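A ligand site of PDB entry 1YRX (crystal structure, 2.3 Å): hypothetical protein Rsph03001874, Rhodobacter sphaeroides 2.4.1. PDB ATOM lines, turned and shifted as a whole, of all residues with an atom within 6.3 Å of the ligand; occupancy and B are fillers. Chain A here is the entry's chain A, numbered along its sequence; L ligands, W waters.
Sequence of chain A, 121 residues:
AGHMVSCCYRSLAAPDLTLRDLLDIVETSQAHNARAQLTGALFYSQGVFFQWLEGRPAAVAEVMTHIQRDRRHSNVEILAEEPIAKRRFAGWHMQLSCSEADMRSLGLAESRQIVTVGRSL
OH of Tyr 9 is in hydrogen-bond range of NE2 of Gln 51 (2.5 Å).
The indole nitrogen (NE1) of Trp 92 lies within hydrogen-bond range of the side-chain amide oxygen (OE1) of Gln 51.
A ring nitrogen (NE2) of His 66 is in hydrogen-bond range of the guanidinium group (NH2) of Arg 69 (3.4 Å).
The side-chain carboxylate (OD1) of Asp 70 is in salt-bridge range of the guanidinium group (NH2) of Arg 72, 2.7 Å away.
The backbone NH (N) of Leu 38 sits at hydrogen-bond distance from the backbone carbonyl oxygen (O) of Asn 33 (2.8 Å).
The side-chain hydroxyl of Ser 29 is in hydrogen-bond range of the backbone carbonyl oxygen of Ile 25 (2.8 Å).
OD1 of Asn 33 sits close to O of Ser 29 (3.3 Å).
The indole nitrogen of Trp 92 lies close to the side-chain amide nitrogen of Asn 33.
Residues that only touch the ligand: Tyr 9 (3.2 Å), Val 63 (3.4 Å), His 73 (3.5 Å), Thr 28 (3.5 Å), Phe 49 (3.5 Å), Ile 25 (3.7 Å), Leu 42 (3.7 Å) and Trp 92 (3.8 Å).
Hydrophobic or aromatic side chains within 4 Å of the ligand: Ile 25, His 32, Leu 42, Phe 49, Val 63, His 66, Ile 67 and His 73.
Of the 26 residues printed, 16 come within 4 Å of the ligand.
The guanidinium group of Arg 72 lies within hydrogen-bond range of an oxygen (O4) of the ligand, at 3.1 Å.
The backbone NH of Ile 67 sits close to an oxygen (O3) of the ligand (3.5 Å).
The side-chain amide oxygen of Gln 51 lies close to an oxygen (O2) of the ligand (2.7 Å).
O3 of the ligand is in hydrogen-bond range of OD1 of Asp 70, at 2.7 Å.
The backbone carbonyl oxygen (O) of His 66 is in hydrogen-bond range of an oxygen (O3) of the ligand (3.5 Å).
A ring nitrogen (ND1) of His 32 lies within hydrogen-bond range of an oxygen (O1) of the ligand (3.1 Å).
OG of Ser 29 lies close to N3 of the ligand.
The side-chain amide oxygen (OD1) of Asn 33 sits at hydrogen-bond distance from a nitrogen (N2) of the ligand, 2.7 Å away.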
ATOM      1  N   TYR A   9      24.476   5.338   0.329  1.00  0.00           N
ATOM      2  CA  TYR A   9      24.324   5.058  -1.094  1.00  0.00           C
ATOM      3  C   TYR A   9      25.162   6.049  -1.878  1.00  0.00           C
ATOM      4  O   TYR A   9      25.479   7.143  -1.379  1.00  0.00           O
ATOM      5  CB  TYR A   9      22.818   5.080  -1.544  1.00  0.00           C
ATOM      6  CG  TYR A   9      22.270   6.483  -1.655  1.00  0.00           C
ATOM      7  CD1 TYR A   9      21.629   7.067  -0.563  1.00  0.00           C
ATOM      8  CD2 TYR A   9      22.460   7.254  -2.815  1.00  0.00           C
ATOM      9  CE1 TYR A   9      21.140   8.378  -0.638  1.00  0.00           C
ATOM     10  CE2 TYR A   9      21.990   8.579  -2.897  1.00  0.00           C
ATOM     11  CZ  TYR A   9      21.320   9.123  -1.790  1.00  0.00           C
ATOM     12  OH  TYR A   9      20.880  10.420  -1.781  1.00  0.00           O
ATOM     13  N   SER A  11      25.095   7.690  -6.094  1.00  0.00           N
ATOM     14  CA  SER A  11      24.253   7.870  -7.255  1.00  0.00           C
ATOM     15  C   SER A  11      24.884   8.845  -8.258  1.00  0.00           C
ATOM     16  O   SER A  11      25.779   9.590  -7.905  1.00  0.00           O
ATOM     17  CB  SER A  11      22.850   8.387  -6.830  1.00  0.00           C
ATOM     18  OG  SER A  11      22.866   9.747  -6.404  1.00  0.00           O
ATOM     19  N   LEU A  17      21.162  18.762 -13.929  1.00  0.00           N
ATOM     20  CA  LEU A  17      20.862  19.282 -12.600  1.00  0.00           C
ATOM     21  C   LEU A  17      21.093  20.789 -12.584  1.00  0.00           C
ATOM     22  O   LEU A  17      22.028  21.309 -13.178  1.00  0.00           O
ATOM     23  CB  LEU A  17      21.704  18.595 -11.537  1.00  0.00           C
ATOM     24  CG  LEU A  17      21.237  18.570 -10.078  1.00  0.00           C
ATOM     25  CD1 LEU A  17      20.034  17.660  -9.928  1.00  0.00           C
ATOM     26  CD2 LEU A  17      22.352  18.082  -9.162  1.00  0.00           C
ATOM     27  N   ASP A  24      15.989  22.900  -3.956  1.00  0.00           N
ATOM     28  CA  ASP A  24      14.887  21.979  -3.533  1.00  0.00           C
ATOM     29  C   ASP A  24      15.402  20.826  -2.671  1.00  0.00           C
ATOM     30  O   ASP A  24      14.844  20.529  -1.618  1.00  0.00           O
ATOM     31  CB  ASP A  24      14.159  21.367  -4.739  1.00  0.00           C
ATOM     32  CG  ASP A  24      13.563  22.400  -5.671  1.00  0.00           C
ATOM     33  OD1 ASP A  24      13.104  23.473  -5.196  1.00  0.00           O
ATOM     34  OD2 ASP A  24      13.531  22.125  -6.893  1.00  0.00           O
ATOM     35  N   ILE A  25      16.440  20.152  -3.123  1.00  0.00           N
ATOM     36  CA  ILE A  25      16.977  19.003  -2.362  1.00  0.00           C
ATOM     37  C   ILE A  25      17.374  19.450  -0.935  1.00  0.00           C
ATOM     38  O   ILE A  25      16.967  18.840   0.044  1.00  0.00           O
ATOM     39  CB  ILE A  25      18.220  18.361  -3.079  1.00  0.00           C
ATOM     40  CG1 ILE A  25      17.787  17.670  -4.353  1.00  0.00           C
ATOM     41  CG2 ILE A  25      19.028  17.403  -2.098  1.00  0.00           C
ATOM     42  CD1 ILE A  25      18.915  17.424  -5.358  1.00  0.00           C
ATOM     43  N   THR A  28      14.221  20.666   1.164  1.00  0.00           N
ATOM     44  CA  THR A  28      13.369  19.526   1.481  1.00  0.00           C
ATOM     45  C   THR A  28      14.020  18.654   2.546  1.00  0.00           C
ATOM     46  O   THR A  28      13.412  18.304   3.554  1.00  0.00           O
ATOM     47  CB  THR A  28      13.061  18.681   0.187  1.00  0.00           C
ATOM     48  OG1 THR A  28      12.474  19.531  -0.798  1.00  0.00           O
ATOM     49  CG2 THR A  28      12.127  17.521   0.511  1.00  0.00           C
ATOM     50  N   SER A  29      15.269  18.295   2.305  1.00  0.00           N
ATOM     51  CA  SER A  29      16.028  17.430   3.219  1.00  0.00           C
ATOM     52  C   SER A  29      16.162  18.007   4.575  1.00  0.00           C
ATOM     53  O   SER A  29      15.939  17.306   5.553  1.00  0.00           O
ATOM     54  CB  SER A  29      17.437  17.174   2.652  1.00  0.00           C
ATOM     55  OG  SER A  29      17.287  16.481   1.449  1.00  0.00           O
ATOM     56  N   GLN A  30      16.562  19.279   4.666  1.00  0.00           N
ATOM     57  CA  GLN A  30      16.682  19.915   5.969  1.00  0.00           C
ATOM     58  C   GLN A  30      15.380  19.844   6.712  1.00  0.00           C
ATOM     59  O   GLN A  30      15.367  19.524   7.898  1.00  0.00           O
ATOM     60  CB  GLN A  30      17.178  21.383   5.881  1.00  0.00           C
ATOM     61  CG  GLN A  30      18.656  21.484   5.525  1.00  0.00           C
ATOM     62  CD  GLN A  30      19.158  22.959   5.325  1.00  0.00           C
ATOM     63  OE1 GLN A  30      18.391  23.869   4.993  1.00  0.00           O
ATOM     64  NE2 GLN A  30      20.466  23.159   5.513  1.00  0.00           N
ATOM     65  N   HIS A  32      12.645  17.819   6.293  1.00  0.00           N
ATOM     66  CA  HIS A  32      12.181  16.472   6.626  1.00  0.00           C
ATOM     67  C   HIS A  32      13.140  15.739   7.602  1.00  0.00           C
ATOM     68  O   HIS A  32      12.703  15.107   8.548  1.00  0.00           O
ATOM     69  CB  HIS A  32      11.953  15.630   5.342  1.00  0.00           C
ATOM     70  CG  HIS A  32      11.527  14.223   5.642  1.00  0.00           C
ATOM     71  ND1 HIS A  32      12.415  13.176   5.720  1.00  0.00           N
ATOM     72  CD2 HIS A  32      10.314  13.710   5.931  1.00  0.00           C
ATOM     73  CE1 HIS A  32      11.766  12.068   6.020  1.00  0.00           C
ATOM     74  NE2 HIS A  32      10.491  12.378   6.181  1.00  0.00           N
ATOM     75  N   ASN A  33      14.447  15.840   7.365  1.00  0.00           N
ATOM     76  CA  ASN A  33      15.438  15.177   8.207  1.00  0.00           C
ATOM     77  C   ASN A  33      15.354  15.686   9.646  1.00  0.00           C
ATOM     78  O   ASN A  33      15.510  14.895  10.575  1.00  0.00           O
ATOM     79  CB  ASN A  33      16.873  15.261   7.611  1.00  0.00           C
ATOM     80  CG  ASN A  33      16.975  14.529   6.269  1.00  0.00           C
ATOM     81  OD1 ASN A  33      15.969  14.003   5.772  1.00  0.00           O
ATOM     82  ND2 ASN A  33      18.195  14.481   5.667  1.00  0.00           N
ATOM     83  N   ARG A  35      12.469  16.936  11.024  1.00  0.00           N
ATOM     84  CA  ARG A  35      11.229  16.372  11.550  1.00  0.00           C
ATOM     85  C   ARG A  35      11.364  14.877  11.928  1.00  0.00           C
ATOM     86  O   ARG A  35      10.914  14.477  12.998  1.00  0.00           O
ATOM     87  CB  ARG A  35      10.039  16.543  10.582  1.00  0.00           C
ATOM     88  CG  ARG A  35       8.795  15.766  11.047  1.00  0.00           C
ATOM     89  CD  ARG A  35       7.685  15.814  10.024  1.00  0.00           C
ATOM     90  NE  ARG A  35       8.253  15.972   8.697  1.00  0.00           N
ATOM     91  CZ  ARG A  35       7.624  15.682   7.564  1.00  0.00           C
ATOM     92  NH1 ARG A  35       8.259  15.877   6.396  1.00  0.00           N
ATOM     93  NH2 ARG A  35       6.367  15.207   7.610  1.00  0.00           N
ATOM     94  N   LEU A  38      16.603  12.390  11.219  1.00  0.00           N
ATOM     95  CA  LEU A  38      17.532  11.743  10.351  1.00  0.00           C
ATOM     96  C   LEU A  38      18.763  12.607  10.309  1.00  0.00           C
ATOM     97  O   LEU A  38      18.707  13.765   9.883  1.00  0.00           O
ATOM     98  CB  LEU A  38      16.958  11.583   8.942  1.00  0.00           C
ATOM     99  CG  LEU A  38      15.797  10.562   8.868  1.00  0.00           C
ATOM    100  CD1 LEU A  38      15.083  10.542   7.515  1.00  0.00           C
ATOM    101  CD2 LEU A  38      16.291   9.158   9.282  1.00  0.00           C
ATOM    102  N   LEU A  42      24.955  14.573   2.940  1.00  0.00           N
ATOM    103  CA  LEU A  42      24.965  14.379   1.518  1.00  0.00           C
ATOM    104  C   LEU A  42      26.180  15.144   0.987  1.00  0.00           C
ATOM    105  O   LEU A  42      26.390  16.312   1.340  1.00  0.00           O
ATOM    106  CB  LEU A  42      23.688  14.947   0.920  1.00  0.00           C
ATOM    107  CG  LEU A  42      23.524  14.992  -0.620  1.00  0.00           C
ATOM    108  CD1 LEU A  42      23.595  13.605  -1.228  1.00  0.00           C
ATOM    109  CD2 LEU A  42      22.150  15.678  -0.966  1.00  0.00           C
ATOM    110  N   PHE A  49      26.562  11.838  -6.264  1.00  0.00           N
ATOM    111  CA  PHE A  49      26.075  12.030  -4.920  1.00  0.00           C
ATOM    112  C   PHE A  49      26.466  10.840  -4.102  1.00  0.00           C
ATOM    113  O   PHE A  49      26.445   9.707  -4.574  1.00  0.00           O
ATOM    114  CB  PHE A  49      24.532  12.170  -4.820  1.00  0.00           C
ATOM    115  CG  PHE A  49      23.979  13.410  -5.451  1.00  0.00           C
ATOM    116  CD1 PHE A  49      24.232  14.666  -4.910  1.00  0.00           C
ATOM    117  CD2 PHE A  49      23.121  13.332  -6.542  1.00  0.00           C
ATOM    118  CE1 PHE A  49      23.640  15.836  -5.467  1.00  0.00           C
ATOM    119  CE2 PHE A  49      22.541  14.498  -7.117  1.00  0.00           C
ATOM    120  CZ  PHE A  49      22.809  15.737  -6.585  1.00  0.00           C
ATOM    121  N   GLN A  51      25.473   9.674  -0.008  1.00  0.00           N
ATOM    122  CA  GLN A  51      24.786  10.124   1.153  1.00  0.00           C
ATOM    123  C   GLN A  51      24.913   9.111   2.263  1.00  0.00           C
ATOM    124  O   GLN A  51      24.868   7.934   2.006  1.00  0.00           O
ATOM    125  CB  GLN A  51      23.297  10.457   0.854  1.00  0.00           C
ATOM    126  CG  GLN A  51      22.556  11.105   2.015  1.00  0.00           C
ATOM    127  CD  GLN A  51      21.175  11.738   1.667  1.00  0.00           C
ATOM    128  OE1 GLN A  51      20.649  12.480   2.475  1.00  0.00           O
ATOM    129  NE2 GLN A  51      20.634  11.492   0.489  1.00  0.00           N
ATOM    130  N   LEU A  53      22.938   8.275   5.811  1.00  0.00           N
ATOM    131  CA  LEU A  53      21.763   8.544   6.643  1.00  0.00           C
ATOM    132  C   LEU A  53      21.604   7.624   7.847  1.00  0.00           C
ATOM    133  O   LEU A  53      21.734   6.432   7.706  1.00  0.00           O
ATOM    134  CB  LEU A  53      20.457   8.422   5.824  1.00  0.00           C
ATOM    135  CG  LEU A  53      19.950   9.696   5.137  1.00  0.00           C
ATOM    136  CD1 LEU A  53      18.840   9.335   4.162  1.00  0.00           C
ATOM    137  CD2 LEU A  53      19.525  10.755   6.189  1.00  0.00           C
ATOM    138  N   VAL A  63      12.547   7.407   3.714  1.00  0.00           N
ATOM    139  CA  VAL A  63      13.199   8.453   2.942  1.00  0.00           C
ATOM    140  C   VAL A  63      13.912   7.808   1.735  1.00  0.00           C
ATOM    141  O   VAL A  63      13.941   8.386   0.637  1.00  0.00           O
ATOM    142  CB  VAL A  63      14.118   9.375   3.809  1.00  0.00           C
ATOM    143  CG1 VAL A  63      15.435   8.701   4.169  1.00  0.00           C
ATOM    144  CG2 VAL A  63      14.408  10.594   3.065  1.00  0.00           C
ATOM    145  N   HIS A  66      11.644   7.355  -1.416  1.00  0.00           N
ATOM    146  CA  HIS A  66      11.609   8.622  -2.127  1.00  0.00           C
ATOM    147  C   HIS A  66      12.894   8.916  -2.847  1.00  0.00           C
ATOM    148  O   HIS A  66      12.876   9.226  -4.009  1.00  0.00           O
ATOM    149  CB  HIS A  66      11.276   9.742  -1.139  1.00  0.00           C
ATOM    150  CG  HIS A  66       9.836   9.731  -0.729  1.00  0.00           C
ATOM    151  ND1 HIS A  66       9.411   9.214   0.471  1.00  0.00           N
ATOM    152  CD2 HIS A  66       8.729  10.158  -1.372  1.00  0.00           C
ATOM    153  CE1 HIS A  66       8.103   9.312   0.562  1.00  0.00           C
ATOM    154  NE2 HIS A  66       7.658   9.877  -0.549  1.00  0.00           N
ATOM    155  N   ILE A  67      14.034   8.864  -2.147  1.00  0.00           N
ATOM    156  CA  ILE A  67      15.321   9.048  -2.790  1.00  0.00           C
ATOM    157  C   ILE A  67      15.499   8.130  -4.003  1.00  0.00           C
ATOM    158  O   ILE A  67      16.013   8.574  -5.031  1.00  0.00           O
ATOM    159  CB  ILE A  67      16.526   8.863  -1.776  1.00  0.00           C
ATOM    160  CG1 ILE A  67      16.455   9.955  -0.676  1.00  0.00           C
ATOM    161  CG2 ILE A  67      17.890   8.810  -2.547  1.00  0.00           C
ATOM    162  CD1 ILE A  67      17.531   9.849   0.416  1.00  0.00           C
ATOM    163  N   GLN A  68      15.096   6.864  -3.895  1.00  0.00           N
ATOM    164  CA  GLN A  68      15.356   5.910  -4.952  1.00  0.00           C
ATOM    165  C   GLN A  68      14.573   6.193  -6.278  1.00  0.00           C
ATOM    166  O   GLN A  68      15.045   5.871  -7.369  1.00  0.00           O
ATOM    167  CB  GLN A  68      15.165   4.453  -4.453  1.00  0.00           C
ATOM    168  CG  GLN A  68      16.452   3.897  -3.763  1.00  0.00           C
ATOM    169  CD  GLN A  68      16.257   2.523  -3.101  1.00  0.00           C
ATOM    170  OE1 GLN A  68      16.752   1.483  -3.601  1.00  0.00           O
ATOM    171  NE2 GLN A  68      15.553   2.505  -1.968  1.00  0.00           N
ATOM    172  N   ARG A  69      13.408   6.843  -6.160  1.00  0.00           N
ATOM    173  CA  ARG A  69      12.623   7.180  -7.332  1.00  0.00           C
ATOM    174  C   ARG A  69      12.798   8.645  -7.735  1.00  0.00           C
ATOM    175  O   ARG A  69      12.135   9.099  -8.634  1.00  0.00           O
ATOM    176  CB  ARG A  69      11.162   6.844  -7.123  1.00  0.00           C
ATOM    177  CG  ARG A  69      10.522   7.641  -6.037  1.00  0.00           C
ATOM    178  CD  ARG A  69       9.213   7.000  -5.675  1.00  0.00           C
ATOM    179  NE  ARG A  69       8.355   7.858  -4.878  1.00  0.00           N
ATOM    180  CZ  ARG A  69       7.385   7.408  -4.097  1.00  0.00           C
ATOM    181  NH1 ARG A  69       7.166   6.097  -3.999  1.00  0.00           N
ATOM    182  NH2 ARG A  69       6.625   8.282  -3.418  1.00  0.00           N
ATOM    183  N   ASP A  70      13.733   9.346  -7.116  1.00  0.00           N
ATOM    184  CA  ASP A  70      13.945  10.766  -7.442  1.00  0.00           C
ATOM    185  C   ASP A  70      14.663  10.912  -8.792  1.00  0.00           C
ATOM    186  O   ASP A  70      15.736  10.310  -9.014  1.00  0.00           O
ATOM    187  CB  ASP A  70      14.766  11.436  -6.354  1.00  0.00           C
ATOM    188  CG  ASP A  70      14.624  12.919  -6.358  1.00  0.00           C
ATOM    189  OD1 ASP A  70      14.344  13.502  -5.305  1.00  0.00           O
ATOM    190  OD2 ASP A  70      14.768  13.511  -7.440  1.00  0.00           O
ATOM    191  N   ARG A  71      14.100  11.730  -9.679  1.00  0.00           N
ATOM    192  CA  ARG A  71      14.609  11.847 -11.054  1.00  0.00           C
ATOM    193  C   ARG A  71      15.818  12.794 -11.186  1.00  0.00           C
ATOM    194  O   ARG A  71      16.411  12.901 -12.263  1.00  0.00           O
ATOM    195  CB  ARG A  71      13.480  12.171 -12.021  1.00  0.00           C
ATOM    196  CG  ARG A  71      12.225  11.300 -11.842  1.00  0.00           C
ATOM    197  CD  ARG A  71      11.168  11.592 -12.884  1.00  0.00           C
ATOM    198  NE  ARG A  71       9.964  10.767 -12.766  1.00  0.00           N
ATOM    199  CZ  ARG A  71       9.779   9.658 -13.474  1.00  0.00           C
ATOM    200  NH1 ARG A  71      10.735   9.269 -14.285  1.00  0.00           N
ATOM    201  NH2 ARG A  71       8.661   8.939 -13.366  1.00  0.00           N
ATOM    202  N   ARG A  72      16.183  13.444 -10.087  1.00  0.00           N
ATOM    203  CA  ARG A  72      17.387  14.283 -10.027  1.00  0.00           C
ATOM    204  C   ARG A  72      18.728  13.526  -9.946  1.00  0.00           C
ATOM    205  O   ARG A  72      19.794  14.136 -10.058  1.00  0.00           O
ATOM    206  CB  ARG A  72      17.250  15.343  -8.911  1.00  0.00           C
ATOM    207  CG  ARG A  72      16.152  16.434  -9.293  1.00  0.00           C
ATOM    208  CD  ARG A  72      15.681  17.245  -8.111  1.00  0.00           C
ATOM    209  NE  ARG A  72      15.117  16.467  -7.017  1.00  0.00           N
ATOM    210  CZ  ARG A  72      14.487  16.978  -5.958  1.00  0.00           C
ATOM    211  NH1 ARG A  72      14.350  18.295  -5.813  1.00  0.00           N
ATOM    212  NH2 ARG A  72      13.970  16.174  -5.024  1.00  0.00           N
ATOM    213  N   HIS A  73      18.660  12.200  -9.803  1.00  0.00           N
ATOM    214  CA  HIS A  73      19.818  11.323  -9.911  1.00  0.00           C
ATOM    215  C   HIS A  73      19.382   9.956 -10.479  1.00  0.00           C
ATOM    216  O   HIS A  73      18.175   9.642 -10.555  1.00  0.00           O
ATOM    217  CB  HIS A  73      20.565  11.171  -8.574  1.00  0.00           C
ATOM    218  CG  HIS A  73      19.749  10.580  -7.466  1.00  0.00           C
ATOM    219  ND1 HIS A  73      20.268  10.323  -6.215  1.00  0.00           N
ATOM    220  CD2 HIS A  73      18.455  10.166  -7.425  1.00  0.00           C
ATOM    221  CE1 HIS A  73      19.324   9.827  -5.446  1.00  0.00           C
ATOM    222  NE2 HIS A  73      18.210   9.732  -6.145  1.00  0.00           N
ATOM    223  N   TRP A  92      22.251  17.181  10.014  1.00  0.00           N
ATOM    224  CA  TRP A  92      22.330  16.862   8.608  1.00  0.00           C
ATOM    225  C   TRP A  92      22.967  18.042   7.904  1.00  0.00           C
ATOM    226  O   TRP A  92      22.784  19.184   8.301  1.00  0.00           O
ATOM    227  CB  TRP A  92      20.932  16.559   8.017  1.00  0.00           C
ATOM    228  CG  TRP A  92      21.008  16.065   6.592  1.00  0.00           C
ATOM    229  CD1 TRP A  92      21.222  14.765   6.168  1.00  0.00           C
ATOM    230  CD2 TRP A  92      20.906  16.851   5.411  1.00  0.00           C
ATOM    231  NE1 TRP A  92      21.276  14.729   4.790  1.00  0.00           N
ATOM    232  CE2 TRP A  92      21.069  16.000   4.307  1.00  0.00           C
ATOM    233  CE3 TRP A  92      20.705  18.211   5.166  1.00  0.00           C
ATOM    234  CZ2 TRP A  92      21.026  16.457   2.986  1.00  0.00           C
ATOM    235  CZ3 TRP A  92      20.684  18.668   3.850  1.00  0.00           C
ATOM    236  CH2 TRP A  92      20.862  17.803   2.790  1.00  0.00           C
HETATM  237  N1  LIG L   1      14.717  13.939   1.030  1.00  0.00           N
HETATM  238  C1  LIG L   1      14.799  13.897   2.388  1.00  0.00           C
HETATM  239  O1  LIG L   1      13.812  14.038   3.049  1.00  0.00           O
HETATM  240  N2  LIG L   1      15.980  13.612   3.065  1.00  0.00           N
HETATM  241  C2  LIG L   1      17.147  13.479   2.361  1.00  0.00           C
HETATM  242  O2  LIG L   1      18.174  13.315   3.021  1.00  0.00           O
HETATM  243  C3  LIG L   1      17.110  13.534   0.977  1.00  0.00           C
HETATM  244  N3  LIG L   1      18.261  13.379   0.239  1.00  0.00           N
HETATM  245  C4  LIG L   1      18.226  13.430  -1.133  1.00  0.00           C
HETATM  246  C5  LIG L   1      19.407  13.284  -1.858  1.00  0.00           C
HETATM  247  C6  LIG L   1      19.392  13.330  -3.243  1.00  0.00           C
HETATM  248  C7  LIG L   1      20.667  13.032  -3.996  1.00  0.00           C
HETATM  249  C8  LIG L   1      18.187  13.519  -3.924  1.00  0.00           C
HETATM  250  C9  LIG L   1      18.180  13.796  -5.423  1.00  0.00           C
HETATM  251  C10 LIG L   1      17.018  13.695  -3.191  1.00  0.00           C
HETATM  252  C11 LIG L   1      17.019  13.647  -1.805  1.00  0.00           C
HETATM  253  N4  LIG L   1      15.828  13.823  -1.076  1.00  0.00           N
HETATM  254  C12 LIG L   1      15.880  13.760   0.304  1.00  0.00           C
HETATM  255  C13 LIG L   1      14.566  14.326  -1.728  1.00  0.00           C
HETATM  256  C14 LIG L   1      13.618  13.117  -1.885  1.00  0.00           C
HETATM  257  O3  LIG L   1      14.119  12.251  -2.894  1.00  0.00           O
HETATM  258  C15 LIG L   1      12.142  13.491  -2.210  1.00  0.00           C
HETATM  259  O4  LIG L   1      12.132  14.416  -3.278  1.00  0.00           O
HETATM  260  C16 LIG L   1      11.393  14.065  -1.020  1.00  0.00           C
HETATM  261  O5  LIG L   1      11.446  13.160   0.062  1.00  0.00           O
HETATM  262  C17 LIG L   1       9.911  14.315  -1.294  1.00  0.00           C
HETATM  263  O6  LIG L   1       9.759  15.723  -1.389  1.00  0.00           O
HETATM  264  P1  LIG L   1       8.354  16.524  -1.210  1.00  0.00           P
HETATM  265  O7  LIG L   1       7.377  16.052  -2.259  1.00  0.00           O
HETATM  266  O8  LIG L   1       8.648  17.985  -1.416  1.00  0.00           O
HETATM  267  O9  LIG L   1       7.787  16.286   0.166  1.00  0.00           O
HETATM  268  O   HOH W   1       7.985  14.247  -3.880  1.00  0.00           O
